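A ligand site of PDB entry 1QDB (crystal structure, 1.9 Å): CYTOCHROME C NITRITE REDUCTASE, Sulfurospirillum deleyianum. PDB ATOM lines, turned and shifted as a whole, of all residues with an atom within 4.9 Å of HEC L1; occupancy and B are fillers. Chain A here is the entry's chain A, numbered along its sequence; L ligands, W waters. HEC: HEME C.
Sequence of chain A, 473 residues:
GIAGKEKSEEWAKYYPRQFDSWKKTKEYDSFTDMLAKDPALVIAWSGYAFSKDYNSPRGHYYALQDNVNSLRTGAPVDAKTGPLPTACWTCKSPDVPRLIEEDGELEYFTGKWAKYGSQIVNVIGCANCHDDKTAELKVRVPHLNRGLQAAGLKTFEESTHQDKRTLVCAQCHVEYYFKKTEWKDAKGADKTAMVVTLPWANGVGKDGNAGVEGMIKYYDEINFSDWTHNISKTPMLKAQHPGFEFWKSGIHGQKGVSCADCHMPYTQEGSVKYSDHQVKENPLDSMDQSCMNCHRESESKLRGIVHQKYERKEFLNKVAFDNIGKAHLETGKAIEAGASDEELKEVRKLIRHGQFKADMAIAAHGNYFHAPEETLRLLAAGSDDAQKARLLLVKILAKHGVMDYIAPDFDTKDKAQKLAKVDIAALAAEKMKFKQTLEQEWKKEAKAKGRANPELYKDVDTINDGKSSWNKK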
ATOM      1  N   TYR A  54      13.514 -25.699  10.260  1.00  0.00           N
ATOM      2  CA  TYR A  54      13.748 -24.687  11.304  1.00  0.00           C
ATOM      3  C   TYR A  54      15.242 -24.598  11.576  1.00  0.00           C
ATOM      4  O   TYR A  54      15.823 -25.493  12.174  1.00  0.00           O
ATOM      5  CB  TYR A  54      12.978 -25.009  12.594  1.00  0.00           C
ATOM      6  CG  TYR A  54      13.334 -24.065  13.723  1.00  0.00           C
ATOM      7  CD1 TYR A  54      13.031 -22.699  13.642  1.00  0.00           C
ATOM      8  CD2 TYR A  54      14.015 -24.508  14.853  1.00  0.00           C
ATOM      9  CE1 TYR A  54      13.400 -21.796  14.656  1.00  0.00           C
ATOM     10  CE2 TYR A  54      14.400 -23.621  15.869  1.00  0.00           C
ATOM     11  CZ  TYR A  54      14.091 -22.277  15.762  1.00  0.00           C
ATOM     12  OH  TYR A  54      14.491 -21.391  16.729  1.00  0.00           O
ATOM     13  N   ASN A  55      15.849 -23.501  11.123  1.00  0.00           N
ATOM     14  CA  ASN A  55      17.278 -23.302  11.307  1.00  0.00           C
ATOM     15  C   ASN A  55      17.557 -22.135  12.243  1.00  0.00           C
ATOM     16  O   ASN A  55      16.685 -21.305  12.504  1.00  0.00           O
ATOM     17  CB  ASN A  55      17.943 -23.001   9.954  1.00  0.00           C
ATOM     18  CG  ASN A  55      17.601 -24.032   8.893  1.00  0.00           C
ATOM     19  OD1 ASN A  55      17.617 -25.234   9.173  1.00  0.00           O
ATOM     20  ND2 ASN A  55      17.247 -23.579   7.701  1.00  0.00           N
ATOM     21  N   SER A  56      18.775 -22.093  12.778  1.00  0.00           N
ATOM     22  CA  SER A  56      19.173 -21.006  13.633  1.00  0.00           C
ATOM     23  C   SER A  56      19.292 -19.765  12.717  1.00  0.00           C
ATOM     24  O   SER A  56      19.381 -19.892  11.490  1.00  0.00           O
ATOM     25  CB  SER A  56      20.512 -21.316  14.296  1.00  0.00           C
ATOM     26  OG  SER A  56      21.531 -21.493  13.334  1.00  0.00           O
ATOM     27  N   PRO A  57      19.294 -18.556  13.303  1.00  0.00           N
ATOM     28  CA  PRO A  57      19.395 -17.356  12.477  1.00  0.00           C
ATOM     29  C   PRO A  57      20.789 -17.132  11.897  1.00  0.00           C
ATOM     30  O   PRO A  57      21.798 -17.535  12.476  1.00  0.00           O
ATOM     31  CB  PRO A  57      19.062 -16.222  13.454  1.00  0.00           C
ATOM     32  CG  PRO A  57      18.518 -16.874  14.674  1.00  0.00           C
ATOM     33  CD  PRO A  57      19.219 -18.203  14.736  1.00  0.00           C
ATOM     34  N   ASP A  66      16.227 -16.474   2.806  1.00  0.00           N
ATOM     35  CA  ASP A  66      16.003 -17.607   3.699  1.00  0.00           C
ATOM     36  C   ASP A  66      14.516 -17.807   3.956  1.00  0.00           C
ATOM     37  O   ASP A  66      14.052 -18.948   4.081  1.00  0.00           O
ATOM     38  CB  ASP A  66      16.779 -17.434   5.001  1.00  0.00           C
ATOM     39  CG  ASP A  66      18.260 -17.600   4.808  1.00  0.00           C
ATOM     40  OD1 ASP A  66      18.688 -18.016   3.707  1.00  0.00           O
ATOM     41  OD2 ASP A  66      19.024 -17.313   5.746  1.00  0.00           O
ATOM     42  N   ASN A  67      13.764 -16.712   3.947  1.00  0.00           N
ATOM     43  CA  ASN A  67      12.311 -16.760   4.132  1.00  0.00           C
ATOM     44  C   ASN A  67      11.716 -17.446   2.892  1.00  0.00           C
ATOM     45  O   ASN A  67      10.685 -18.124   2.966  1.00  0.00           O
ATOM     46  CB  ASN A  67      11.758 -15.341   4.293  1.00  0.00           C
ATOM     47  CG  ASN A  67      10.243 -15.297   4.350  1.00  0.00           C
ATOM     48  OD1 ASN A  67       9.585 -15.020   3.358  1.00  0.00           O
ATOM     49  ND2 ASN A  67       9.683 -15.517   5.534  1.00  0.00           N
ATOM     50  N   SER A  70      13.063 -21.459   2.900  1.00  0.00           N
ATOM     51  CA  SER A  70      12.489 -22.294   3.943  1.00  0.00           C
ATOM     52  C   SER A  70      11.333 -23.155   3.478  1.00  0.00           C
ATOM     53  O   SER A  70      10.446 -22.676   2.766  1.00  0.00           O
ATOM     54  CB  SER A  70      12.033 -21.422   5.104  1.00  0.00           C
ATOM     55  OG  SER A  70      11.438 -22.192   6.130  1.00  0.00           O
ATOM     56  N   ARG A  72       9.000 -23.957   5.190  1.00  0.00           N
ATOM     57  CA  ARG A  72       7.800 -23.409   5.819  1.00  0.00           C
ATOM     58  C   ARG A  72       6.877 -22.620   4.887  1.00  0.00           C
ATOM     59  O   ARG A  72       5.651 -22.728   4.987  1.00  0.00           O
ATOM     60  CB  ARG A  72       8.162 -22.556   7.059  1.00  0.00           C
ATOM     61  CG  ARG A  72       8.928 -23.329   8.140  1.00  0.00           C
ATOM     62  CD  ARG A  72       8.615 -22.846   9.553  1.00  0.00           C
ATOM     63  NE  ARG A  72       9.069 -21.483   9.857  1.00  0.00           N
ATOM     64  CZ  ARG A  72      10.334 -21.131  10.103  1.00  0.00           C
ATOM     65  NH1 ARG A  72      11.311 -22.026  10.074  1.00  0.00           N
ATOM     66  NH2 ARG A  72      10.605 -19.867  10.452  1.00  0.00           N
ATOM     67  N   THR A  73       7.450 -21.829   3.993  1.00  0.00           N
ATOM     68  CA  THR A  73       6.644 -21.045   3.058  1.00  0.00           C
ATOM     69  C   THR A  73       6.097 -21.895   1.916  1.00  0.00           C
ATOM     70  O   THR A  73       5.240 -21.446   1.154  1.00  0.00           O
ATOM     71  CB  THR A  73       7.411 -19.825   2.509  1.00  0.00           C
ATOM     72  OG1 THR A  73       8.768 -20.178   2.197  1.00  0.00           O
ATOM     73  CG2 THR A  73       7.378 -18.683   3.530  1.00  0.00           C
ATOM     74  N   LEU A  84       1.398 -20.501   3.659  1.00  0.00           N
ATOM     75  CA  LEU A  84       1.447 -19.298   4.512  1.00  0.00           C
ATOM     76  C   LEU A  84       1.029 -17.970   3.867  1.00  0.00           C
ATOM     77  O   LEU A  84       1.201 -17.782   2.657  1.00  0.00           O
ATOM     78  CB  LEU A  84       2.848 -19.187   5.133  1.00  0.00           C
ATOM     79  CG  LEU A  84       3.298 -20.449   5.897  1.00  0.00           C
ATOM     80  CD1 LEU A  84       4.657 -20.238   6.484  1.00  0.00           C
ATOM     81  CD2 LEU A  84       2.289 -20.797   6.989  1.00  0.00           C
ATOM     82  N   ALA A  87       1.660 -12.013   5.891  1.00  0.00           N
ATOM     83  CA  ALA A  87       2.314 -11.644   7.147  1.00  0.00           C
ATOM     84  C   ALA A  87       3.729 -12.201   7.299  1.00  0.00           C
ATOM     85  O   ALA A  87       4.545 -11.638   8.035  1.00  0.00           O
ATOM     86  CB  ALA A  87       1.447 -12.052   8.320  1.00  0.00           C
ATOM     87  N   CYS A  88       4.039 -13.285   6.584  1.00  0.00           N
ATOM     88  CA  CYS A  88       5.368 -13.882   6.662  1.00  0.00           C
ATOM     89  C   CYS A  88       6.474 -13.021   6.046  1.00  0.00           C
ATOM     90  O   CYS A  88       7.658 -13.301   6.220  1.00  0.00           O
ATOM     91  CB  CYS A  88       5.381 -15.291   6.054  1.00  0.00           C
ATOM     92  SG  CYS A  88       4.579 -16.507   7.103  1.00  0.00           S
ATOM     93  N   THR A  90       6.532  -9.614   6.590  1.00  0.00           N
ATOM     94  CA  THR A  90       6.627  -8.503   7.543  1.00  0.00           C
ATOM     95  C   THR A  90       7.940  -8.074   8.178  1.00  0.00           C
ATOM     96  O   THR A  90       8.206  -6.861   8.296  1.00  0.00           O
ATOM     97  CB  THR A  90       5.560  -8.636   8.641  1.00  0.00           C
ATOM     98  OG1 THR A  90       4.330  -9.006   8.021  1.00  0.00           O
ATOM     99  CG2 THR A  90       5.340  -7.301   9.363  1.00  0.00           C
ATOM    100  N   CYS A  91       8.777  -9.029   8.553  1.00  0.00           N
ATOM    101  CA  CYS A  91      10.037  -8.703   9.194  1.00  0.00           C
ATOM    102  C   CYS A  91      11.233  -9.132   8.385  1.00  0.00           C
ATOM    103  O   CYS A  91      12.261  -9.526   8.929  1.00  0.00           O
ATOM    104  CB  CYS A  91      10.070  -9.358  10.580  1.00  0.00           C
ATOM    105  SG  CYS A  91       8.598  -9.020  11.573  1.00  0.00           S
ATOM    106  N   LYS A  92      11.131  -8.978   7.061  1.00  0.00           N
ATOM    107  CA  LYS A  92      12.216  -9.408   6.197  1.00  0.00           C
ATOM    108  C   LYS A  92      12.613  -8.364   5.150  1.00  0.00           C
ATOM    109  O   LYS A  92      13.641  -8.523   4.506  1.00  0.00           O
ATOM    110  CB  LYS A  92      11.811 -10.704   5.476  1.00  0.00           C
ATOM    111  CG  LYS A  92      11.298 -11.843   6.387  1.00  0.00           C
ATOM    112  CD  LYS A  92      12.428 -12.484   7.184  1.00  0.00           C
ATOM    113  CE  LYS A  92      11.985 -13.750   7.938  1.00  0.00           C
ATOM    114  NZ  LYS A  92      11.098 -13.567   9.134  1.00  0.00           N
ATOM    115  N   HIS A 143       2.569  -2.647  13.967  1.00  0.00           N
ATOM    116  CA  HIS A 143       2.389  -3.668  15.001  1.00  0.00           C
ATOM    117  C   HIS A 143       3.149  -3.336  16.291  1.00  0.00           C
ATOM    118  O   HIS A 143       2.631  -3.585  17.388  1.00  0.00           O
ATOM    119  CB  HIS A 143       2.713  -5.095  14.503  1.00  0.00           C
ATOM    120  CG  HIS A 143       4.139  -5.318  14.113  1.00  0.00           C
ATOM    121  ND1 HIS A 143       4.542  -5.422  12.800  1.00  0.00           N
ATOM    122  CD2 HIS A 143       5.259  -5.479  14.853  1.00  0.00           C
ATOM    123  CE1 HIS A 143       5.843  -5.619  12.748  1.00  0.00           C
ATOM    124  NE2 HIS A 143       6.307  -5.657  13.991  1.00  0.00           N
ATOM    125  N   GLN A 171      11.026  -4.254  16.571  1.00  0.00           N
ATOM    126  CA  GLN A 171       9.983  -4.256  15.541  1.00  0.00           C
ATOM    127  C   GLN A 171       9.904  -5.629  14.874  1.00  0.00           C
ATOM    128  O   GLN A 171       8.893  -5.966  14.254  1.00  0.00           O
ATOM    129  CB  GLN A 171      10.199  -3.143  14.514  1.00  0.00           C
ATOM    130  CG  GLN A 171      11.516  -3.168  13.815  1.00  0.00           C
ATOM    131  CD  GLN A 171      11.651  -2.058  12.789  1.00  0.00           C
ATOM    132  OE1 GLN A 171      10.681  -1.694  12.110  1.00  0.00           O
ATOM    133  NE2 GLN A 171      12.856  -1.529  12.639  1.00  0.00           N
ATOM    134  N   CYS A 172      10.952  -6.426  15.028  1.00  0.00           N
ATOM    135  CA  CYS A 172      11.013  -7.784  14.466  1.00  0.00           C
ATOM    136  C   CYS A 172      11.303  -8.885  15.489  1.00  0.00           C
ATOM    137  O   CYS A 172      10.692  -9.946  15.442  1.00  0.00           O
ATOM    138  CB  CYS A 172      12.089  -7.847  13.380  1.00  0.00           C
ATOM    139  SG  CYS A 172      11.783  -6.771  11.963  1.00  0.00           S
ATOM    140  N   HIS A 173      12.269  -8.631  16.379  1.00  0.00           N
ATOM    141  CA  HIS A 173      12.667  -9.628  17.381  1.00  0.00           C
ATOM    142  C   HIS A 173      11.757  -9.692  18.596  1.00  0.00           C
ATOM    143  O   HIS A 173      12.190  -9.455  19.735  1.00  0.00           O
ATOM    144  CB  HIS A 173      14.122  -9.400  17.793  1.00  0.00           C
ATOM    145  CG  HIS A 173      15.126  -9.703  16.710  1.00  0.00           C
ATOM    146  ND1 HIS A 173      15.858 -10.862  16.641  1.00  0.00           N
ATOM    147  CD2 HIS A 173      15.511  -8.962  15.639  1.00  0.00           C
ATOM    148  CE1 HIS A 173      16.665 -10.794  15.555  1.00  0.00           C
ATOM    149  NE2 HIS A 173      16.495  -9.661  14.908  1.00  0.00           N
ATOM    150  N   VAL A 174      10.503 -10.041  18.337  1.00  0.00           N
ATOM    151  CA  VAL A 174       9.472 -10.153  19.355  1.00  0.00           C
ATOM    152  C   VAL A 174       8.559 -11.347  19.031  1.00  0.00           C
ATOM    153  O   VAL A 174       8.580 -11.877  17.908  1.00  0.00           O
ATOM    154  CB  VAL A 174       8.579  -8.886  19.386  1.00  0.00           C
ATOM    155  CG1 VAL A 174       9.350  -7.690  19.958  1.00  0.00           C
ATOM    156  CG2 VAL A 174       8.067  -8.570  17.982  1.00  0.00           C
ATOM    157  N   TYR A 176       4.846 -12.986  18.461  1.00  0.00           N
ATOM    158  CA  TYR A 176       3.647 -12.461  17.823  1.00  0.00           C
ATOM    159  C   TYR A 176       2.719 -13.597  17.402  1.00  0.00           C
ATOM    160  O   TYR A 176       3.086 -14.756  17.472  1.00  0.00           O
ATOM    161  CB  TYR A 176       4.059 -11.731  16.534  1.00  0.00           C
ATOM    162  CG  TYR A 176       4.584 -12.689  15.479  1.00  0.00           C
ATOM    163  CD1 TYR A 176       5.926 -13.100  15.469  1.00  0.00           C
ATOM    164  CD2 TYR A 176       3.717 -13.271  14.536  1.00  0.00           C
ATOM    165  CE1 TYR A 176       6.380 -14.071  14.572  1.00  0.00           C
ATOM    166  CE2 TYR A 176       4.164 -14.236  13.643  1.00  0.00           C
ATOM    167  CZ  TYR A 176       5.485 -14.639  13.663  1.00  0.00           C
ATOM    168  OH  TYR A 176       5.893 -15.622  12.787  1.00  0.00           O
ATOM    169  N   PHE A 178      -0.820 -14.301  14.394  1.00  0.00           N
ATOM    170  CA  PHE A 178      -1.581 -13.733  13.282  1.00  0.00           C
ATOM    171  C   PHE A 178      -3.023 -13.608  13.733  1.00  0.00           C
ATOM    172  O   PHE A 178      -3.675 -14.603  14.045  1.00  0.00           O
ATOM    173  CB  PHE A 178      -1.509 -14.643  12.060  1.00  0.00           C
ATOM    174  CG  PHE A 178      -0.141 -14.748  11.451  1.00  0.00           C
ATOM    175  CD1 PHE A 178       0.829 -13.782  11.689  1.00  0.00           C
ATOM    176  CD2 PHE A 178       0.172 -15.819  10.619  1.00  0.00           C
ATOM    177  CE1 PHE A 178       2.088 -13.877  11.115  1.00  0.00           C
ATOM    178  CE2 PHE A 178       1.438 -15.921  10.042  1.00  0.00           C
ATOM    179  CZ  PHE A 178       2.397 -14.958  10.293  1.00  0.00           C
ATOM    180  N   VAL A 196      -0.191  -9.417  11.888  1.00  0.00           N
ATOM    181  CA  VAL A 196       0.857  -9.619  12.886  1.00  0.00           C
ATOM    182  C   VAL A 196       0.469  -8.817  14.125  1.00  0.00           C
ATOM    183  O   VAL A 196       0.276  -7.607  14.051  1.00  0.00           O
ATOM    184  CB  VAL A 196       2.239  -9.155  12.371  1.00  0.00           C
ATOM    185  CG1 VAL A 196       3.268  -9.139  13.507  1.00  0.00           C
ATOM    186  CG2 VAL A 196       2.729 -10.077  11.272  1.00  0.00           C
ATOM    187  N   HIS A 241      10.896 -16.139  18.554  1.00  0.00           N
ATOM    188  CA  HIS A 241      11.932 -15.183  18.943  1.00  0.00           C
ATOM    189  C   HIS A 241      11.495 -13.986  19.795  1.00  0.00           C
ATOM    190  O   HIS A 241      11.398 -12.857  19.299  1.00  0.00           O
ATOM    191  CB  HIS A 241      12.603 -14.675  17.662  1.00  0.00           C
ATOM    192  CG  HIS A 241      11.625 -14.401  16.556  1.00  0.00           C
ATOM    193  ND1 HIS A 241      10.642 -13.442  16.649  1.00  0.00           N
ATOM    194  CD2 HIS A 241      11.418 -15.040  15.368  1.00  0.00           C
ATOM    195  CE1 HIS A 241       9.861 -13.498  15.580  1.00  0.00           C
ATOM    196  NE2 HIS A 241      10.317 -14.458  14.795  1.00  0.00           N
ATOM    197  N   ALA A 363      13.115 -19.946  21.963  1.00  0.00           N
ATOM    198  CA  ALA A 363      12.787 -19.320  20.676  1.00  0.00           C
ATOM    199  C   ALA A 363      13.614 -18.089  20.309  1.00  0.00           C
ATOM    200  O   ALA A 363      13.730 -17.759  19.126  1.00  0.00           O
ATOM    201  CB  ALA A 363      11.302 -19.019  20.607  1.00  0.00           C
ATOM    202  N   HIS A 365      17.198 -17.088  20.407  1.00  0.00           N
ATOM    203  CA  HIS A 365      18.479 -17.737  20.646  1.00  0.00           C
ATOM    204  C   HIS A 365      19.427 -17.096  21.649  1.00  0.00           C
ATOM    205  O   HIS A 365      20.171 -17.800  22.323  1.00  0.00           O
ATOM    206  CB  HIS A 365      19.163 -18.056  19.316  1.00  0.00           C
ATOM    207  CG  HIS A 365      18.376 -18.991  18.458  1.00  0.00           C
ATOM    208  ND1 HIS A 365      18.473 -20.361  18.565  1.00  0.00           N
ATOM    209  CD2 HIS A 365      17.407 -18.755  17.534  1.00  0.00           C
ATOM    210  CE1 HIS A 365      17.597 -20.935  17.747  1.00  0.00           C
ATOM    211  NE2 HIS A 365      16.951 -19.974  17.111  1.00  0.00           N
HETATM  212 FE   HEC L   1      10.681 -14.862  10.491  1.00  0.00          FE
HETATM  213  CHA HEC L   1      13.960 -15.680  11.145  1.00  0.00           C
HETATM  214  CHB HEC L   1      10.479 -17.328   8.256  1.00  0.00           C
HETATM  215  CHC HEC L   1       7.238 -14.380  10.261  1.00  0.00           C
HETATM  216  CHD HEC L   1      10.907 -12.334  12.587  1.00  0.00           C
HETATM  217  NA  HEC L   1      11.957 -16.159   9.839  1.00  0.00           N
HETATM  218  C1A HEC L   1      13.285 -16.372  10.166  1.00  0.00           C
HETATM  219  C2A HEC L   1      13.861 -17.439   9.377  1.00  0.00           C
HETATM  220  C3A HEC L   1      12.885 -17.883   8.584  1.00  0.00           C
HETATM  221  C4A HEC L   1      11.703 -17.109   8.864  1.00  0.00           C
HETATM  222  CMA HEC L   1      13.025 -18.934   7.483  1.00  0.00           C
HETATM  223  CAA HEC L   1      15.280 -17.972   9.470  1.00  0.00           C
HETATM  224  CBA HEC L   1      15.379 -18.993  10.607  1.00  0.00           C
HETATM  225  CGA HEC L   1      14.563 -20.244  10.335  1.00  0.00           C
HETATM  226  O1A HEC L   1      14.995 -21.066   9.511  1.00  0.00           O
HETATM  227  O2A HEC L   1      13.480 -20.401  10.931  1.00  0.00           O
HETATM  228  NB  HEC L   1       9.178 -15.652   9.487  1.00  0.00           N
HETATM  229  C1B HEC L   1       9.282 -16.710   8.568  1.00  0.00           C
HETATM  230  C2B HEC L   1       7.971 -17.128   8.099  1.00  0.00           C
HETATM  231  C3B HEC L   1       7.043 -16.328   8.703  1.00  0.00           C
HETATM  232  C4B HEC L   1       7.803 -15.408   9.542  1.00  0.00           C
HETATM  233  CMB HEC L   1       7.647 -18.306   7.161  1.00  0.00           C
HETATM  234  CAB HEC L   1       5.665 -16.437   8.630  1.00  0.00           C
HETATM  235  CBB HEC L   1       4.935 -17.255   9.540  1.00  0.00           C
HETATM  236  NC  HEC L   1       9.353 -13.628  11.215  1.00  0.00           N
HETATM  237  C1C HEC L   1       8.008 -13.512  11.049  1.00  0.00           C
HETATM  238  C2C HEC L   1       7.480 -12.293  11.663  1.00  0.00           C
HETATM  239  C3C HEC L   1       8.531 -11.625  12.253  1.00  0.00           C
HETATM  240  C4C HEC L   1       9.673 -12.516  12.003  1.00  0.00           C
HETATM  241  CMC HEC L   1       6.008 -11.906  11.650  1.00  0.00           C
HETATM  242  CAC HEC L   1       8.537 -10.335  12.862  1.00  0.00           C
HETATM  243  CBC HEC L   1       7.520  -9.860  13.763  1.00  0.00           C
HETATM  244  ND  HEC L   1      12.103 -14.205  11.664  1.00  0.00           N
HETATM  245  C1D HEC L   1      12.012 -13.117  12.478  1.00  0.00           C
HETATM  246  C2D HEC L   1      13.219 -12.923  13.226  1.00  0.00           C
HETATM  247  C3D HEC L   1      14.060 -13.922  12.890  1.00  0.00           C
HETATM  248  C4D HEC L   1      13.372 -14.685  11.882  1.00  0.00           C
HETATM  249  CMD HEC L   1      13.455 -11.828  14.261  1.00  0.00           C
HETATM  250  CAD HEC L   1      15.426 -14.188  13.472  1.00  0.00           C
HETATM  251  CBD HEC L   1      15.445 -14.772  14.895  1.00  0.00           C
HETATM  252  CGD HEC L   1      15.159 -16.280  14.932  1.00  0.00           C
HETATM  253  O1D HEC L   1      15.150 -16.935  13.866  1.00  0.00           O
HETATM  254  O2D HEC L   1      14.959 -16.810  16.056  1.00  0.00           O
HETATM  255 FE   HEC L   2      17.720  -9.102  13.458  1.00  0.00          FE
HETATM  256  CHA HEC L   2      18.978 -12.034  12.476  1.00  0.00           C
HETATM  257  CHB HEC L   2      20.069  -8.825  15.958  1.00  0.00           C
HETATM  258  CHC HEC L   2      16.980  -5.880  13.812  1.00  0.00           C
HETATM  259  CHD HEC L   2      14.953  -9.613  11.455  1.00  0.00           C
HETATM  260  NA  HEC L   2      19.191 -10.161  14.060  1.00  0.00           N
HETATM  261  C1A HEC L   2      19.640 -11.358  13.486  1.00  0.00           C
HETATM  262  C2A HEC L   2      20.885 -11.773  14.091  1.00  0.00           C
HETATM  263  C3A HEC L   2      21.112 -10.926  15.118  1.00  0.00           C
HETATM  264  C4A HEC L   2      20.081  -9.931  15.096  1.00  0.00           C
HETATM  265  CMA HEC L   2      22.234 -11.003  16.155  1.00  0.00           C
HETATM  266  CAA HEC L   2      21.902 -12.807  13.617  1.00  0.00           C
HETATM  267  CBA HEC L   2      22.544 -12.483  12.267  1.00  0.00           C
HETATM  268  CGA HEC L   2      23.186 -11.110  12.225  1.00  0.00           C
HETATM  269  O1A HEC L   2      23.980 -10.810  13.137  1.00  0.00           O
HETATM  270  O2A HEC L   2      22.908 -10.336  11.283  1.00  0.00           O
HETATM  271  NB  HEC L   2      18.326  -7.670  14.694  1.00  0.00           N
HETATM  272  C1B HEC L   2      19.213  -7.751  15.734  1.00  0.00           C
HETATM  273  C2B HEC L   2      19.381  -6.456  16.373  1.00  0.00           C
HETATM  274  C3B HEC L   2      18.595  -5.552  15.729  1.00  0.00           C
HETATM  275  C4B HEC L   2      17.934  -6.343  14.683  1.00  0.00           C
HETATM  276  CMB HEC L   2      20.301  -6.314  17.579  1.00  0.00           C
HETATM  277  CAB HEC L   2      18.499  -4.155  15.912  1.00  0.00           C
HETATM  278  CBB HEC L   2      19.648  -3.341  15.779  1.00  0.00           C
HETATM  279  NC  HEC L   2      16.306  -8.015  12.751  1.00  0.00           N
HETATM  280  C1C HEC L   2      16.214  -6.622  12.921  1.00  0.00           C
HETATM  281  C2C HEC L   2      15.076  -6.088  12.267  1.00  0.00           C
HETATM  282  C3C HEC L   2      14.409  -7.132  11.688  1.00  0.00           C
HETATM  283  C4C HEC L   2      15.197  -8.337  11.969  1.00  0.00           C
HETATM  284  CMC HEC L   2      14.743  -4.591  12.170  1.00  0.00           C
HETATM  285  CAC HEC L   2      13.208  -7.060  10.989  1.00  0.00           C
HETATM  286  CBC HEC L   2      13.002  -6.288   9.786  1.00  0.00           C
HETATM  287  ND  HEC L   2      17.055 -10.574  12.271  1.00  0.00           N
HETATM  288  C1D HEC L   2      15.867 -10.658  11.573  1.00  0.00           C
HETATM  289  C2D HEC L   2      15.840 -11.869  10.745  1.00  0.00           C
HETATM  290  C3D HEC L   2      16.976 -12.528  10.991  1.00  0.00           C
HETATM  291  C4D HEC L   2      17.748 -11.706  11.938  1.00  0.00           C
HETATM  292  CMD HEC L   2      14.764 -12.209   9.741  1.00  0.00           C
HETATM  293  CAD HEC L   2      17.359 -13.900  10.449  1.00  0.00           C
HETATM  294  CBD HEC L   2      17.907 -13.765   9.026  1.00  0.00           C
HETATM  295  CGD HEC L   2      18.323 -15.100   8.398  1.00  0.00           C
HETATM  296  O1D HEC L   2      18.406 -16.130   9.113  1.00  0.00           O
HETATM  297  O2D HEC L   2      18.594 -15.112   7.174  1.00  0.00           O
HETATM  298  O   HOH W   1      16.671 -20.621   7.438  1.00  0.00           O
HETATM  299  O   HOH W   2      13.486 -22.731   7.709  1.00  0.00           O
HETATM  300  O   HOH W   3      16.412 -15.474  17.981  1.00  0.00           O
HETATM  301  O   HOH W   4      15.905 -19.565  14.513  1.00  0.00           O
HETATM  302  O   HOH W   5       7.066 -19.645  10.421  1.00  0.00           O
HETATM  303  O   HOH W   6      12.531 -18.445  12.915  1.00  0.00           O
HETATM  304  O   HOH W   7       4.027 -19.029  12.274  1.00  0.00           O
HETATM  305  O   HOH W   8      13.629 -18.942  16.720  1.00  0.00           O
HETATM  306  O   HOH W   9      14.845 -15.191   7.482  1.00  0.00           O
HETATM  307  O   HOH W  10       8.473 -11.846   8.455  1.00  0.00           O
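Water W8 lies within hydrogen-bond range of OH of Tyr 54 (2.6 Å), O2D of HEC L1 (2.6 Å) and O of Ala 363 (2.7 Å). Water W1 lies within hydrogen-bond range of O1A of HEC L1 (2.7 Å) and ND2 of Asn 55 (3.0 Å). Water W3 bridges O2D of HEC L1 (2.8 Å) and N of His 365 (3.0 Å). Water W4 lies within hydrogen-bond range of the backbone carbonyl oxygen (O) of Asn 55 (2.8 Å), an oxygen (O1D) of HEC L1 (2.8 Å), a ring nitrogen (NE2) of His 365 (2.8 Å) and the side-chain hydroxyl (OH) of Tyr 54 (3.2 Å). Water W2 lies within hydrogen-bond range of the side-chain hydroxyl (OG) of Ser 70, an oxygen (O1A) of HEC L1 and the guanidinium group (NH1) of Arg 72. Water W6 lies within hydrogen-bond range of O2A of HEC L1 (2.9 Å) and NH2 of Arg 72 (3.4 Å).
CAC of HEC L2 is bonded to SG of Cys 172, 1.8 Å away. SG of Cys 91 is bonded to CAC of HEC L1, at 1.8 Å. NH1 of Arg 72 is in salt-bridge range of O2A of HEC L1, 2.8 Å away. N of Asn 55 lies within hydrogen-bond range of O1A of HEC L1 (3.0 Å). The side-chain carboxylate of Asp 66 sits close to an oxygen (O2D) of HEC L2, 2.7 Å away. The side-chain amino group of Lys 92 binds an iron atom (FE) of HEC L1. An iron atom (FE) of HEC L2 is bound by a ring nitrogen (NE2) of His 173, 2.0 Å away. The side-chain sulfur (SG) of Cys 88 is bonded to a carbon (CAB) of HEC L1, at 1.9 Å.
The backbone carbonyl oxygen (O) of Ala 363 sits close to an oxygen (O2D) of HEC L1 (3.4 Å). Tyr 54 touches HEC L1 (CD1 to O2A, 3.6 Å). Pro 57 touches HEC L1 (CG to CGD, 3.4 Å). Asp 66 touches HEC L1. Asn 67 touches HEC L1. Ser 70 touches HEC L1 (CB to CMA, 3.6 Å). Thr 73 touches HEC L1 (CG2 to CMB, 3.7 Å). CD1 of Leu 84 touches CMB of HEC L1, 3.6 Å away. Ala 87 touches HEC L1. Cys 172 touches HEC L1 (O to CAC, 3.4 Å). His 173 touches HEC L1 (ND1 to CMD, 3.5 Å). OH of Tyr 176 touches CHC of HEC L1 (3.1 Å). Phe 178 touches HEC L1 (CZ to CBB, 3.5 Å). Val 196 touches HEC L1. NE2 of His 241 touches CHD of HEC L1, 3.1 Å away. His 365 touches HEC L1. Hydrophobic or aromatic side chains within 4 Å of HEC L1: Tyr 54, Pro 57, Leu 84, His 173, Tyr 176, Phe 178, Val 196, His 241 and His 365. Of the 26 residues printed, 21 come within 4 Å of HEC L1.
The backbone carbonyl oxygen (O) of Ala 363 sits close to the backbone NH (N) of His 241 (3.3 Å). O of Ser 70 is in hydrogen-bond range of OG1 of Thr 73. N of Arg 72 lies close to OG of Ser 70, at 3.2 Å. The side-chain amide nitrogen (ND2) of Asn 67 is in hydrogen-bond range of the backbone carbonyl oxygen (O) of Cys 88, at 3.1 Å. The side-chain hydroxyl (OG1) of Thr 90 sits at hydrogen-bond distance from the backbone carbonyl oxygen (O) of Ala 87. A ring nitrogen (NE2) of His 365 is in hydrogen-bond range of the side-chain hydroxyl (OH) of Tyr 54 (2.9 Å). OG1 of Thr 73 lies within hydrogen-bond range of O of Asn 67 (2.9 Å). A ring nitrogen (ND1) of His 241 is in hydrogen-bond range of the backbone carbonyl oxygen of Val 174 (2.9 Å).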
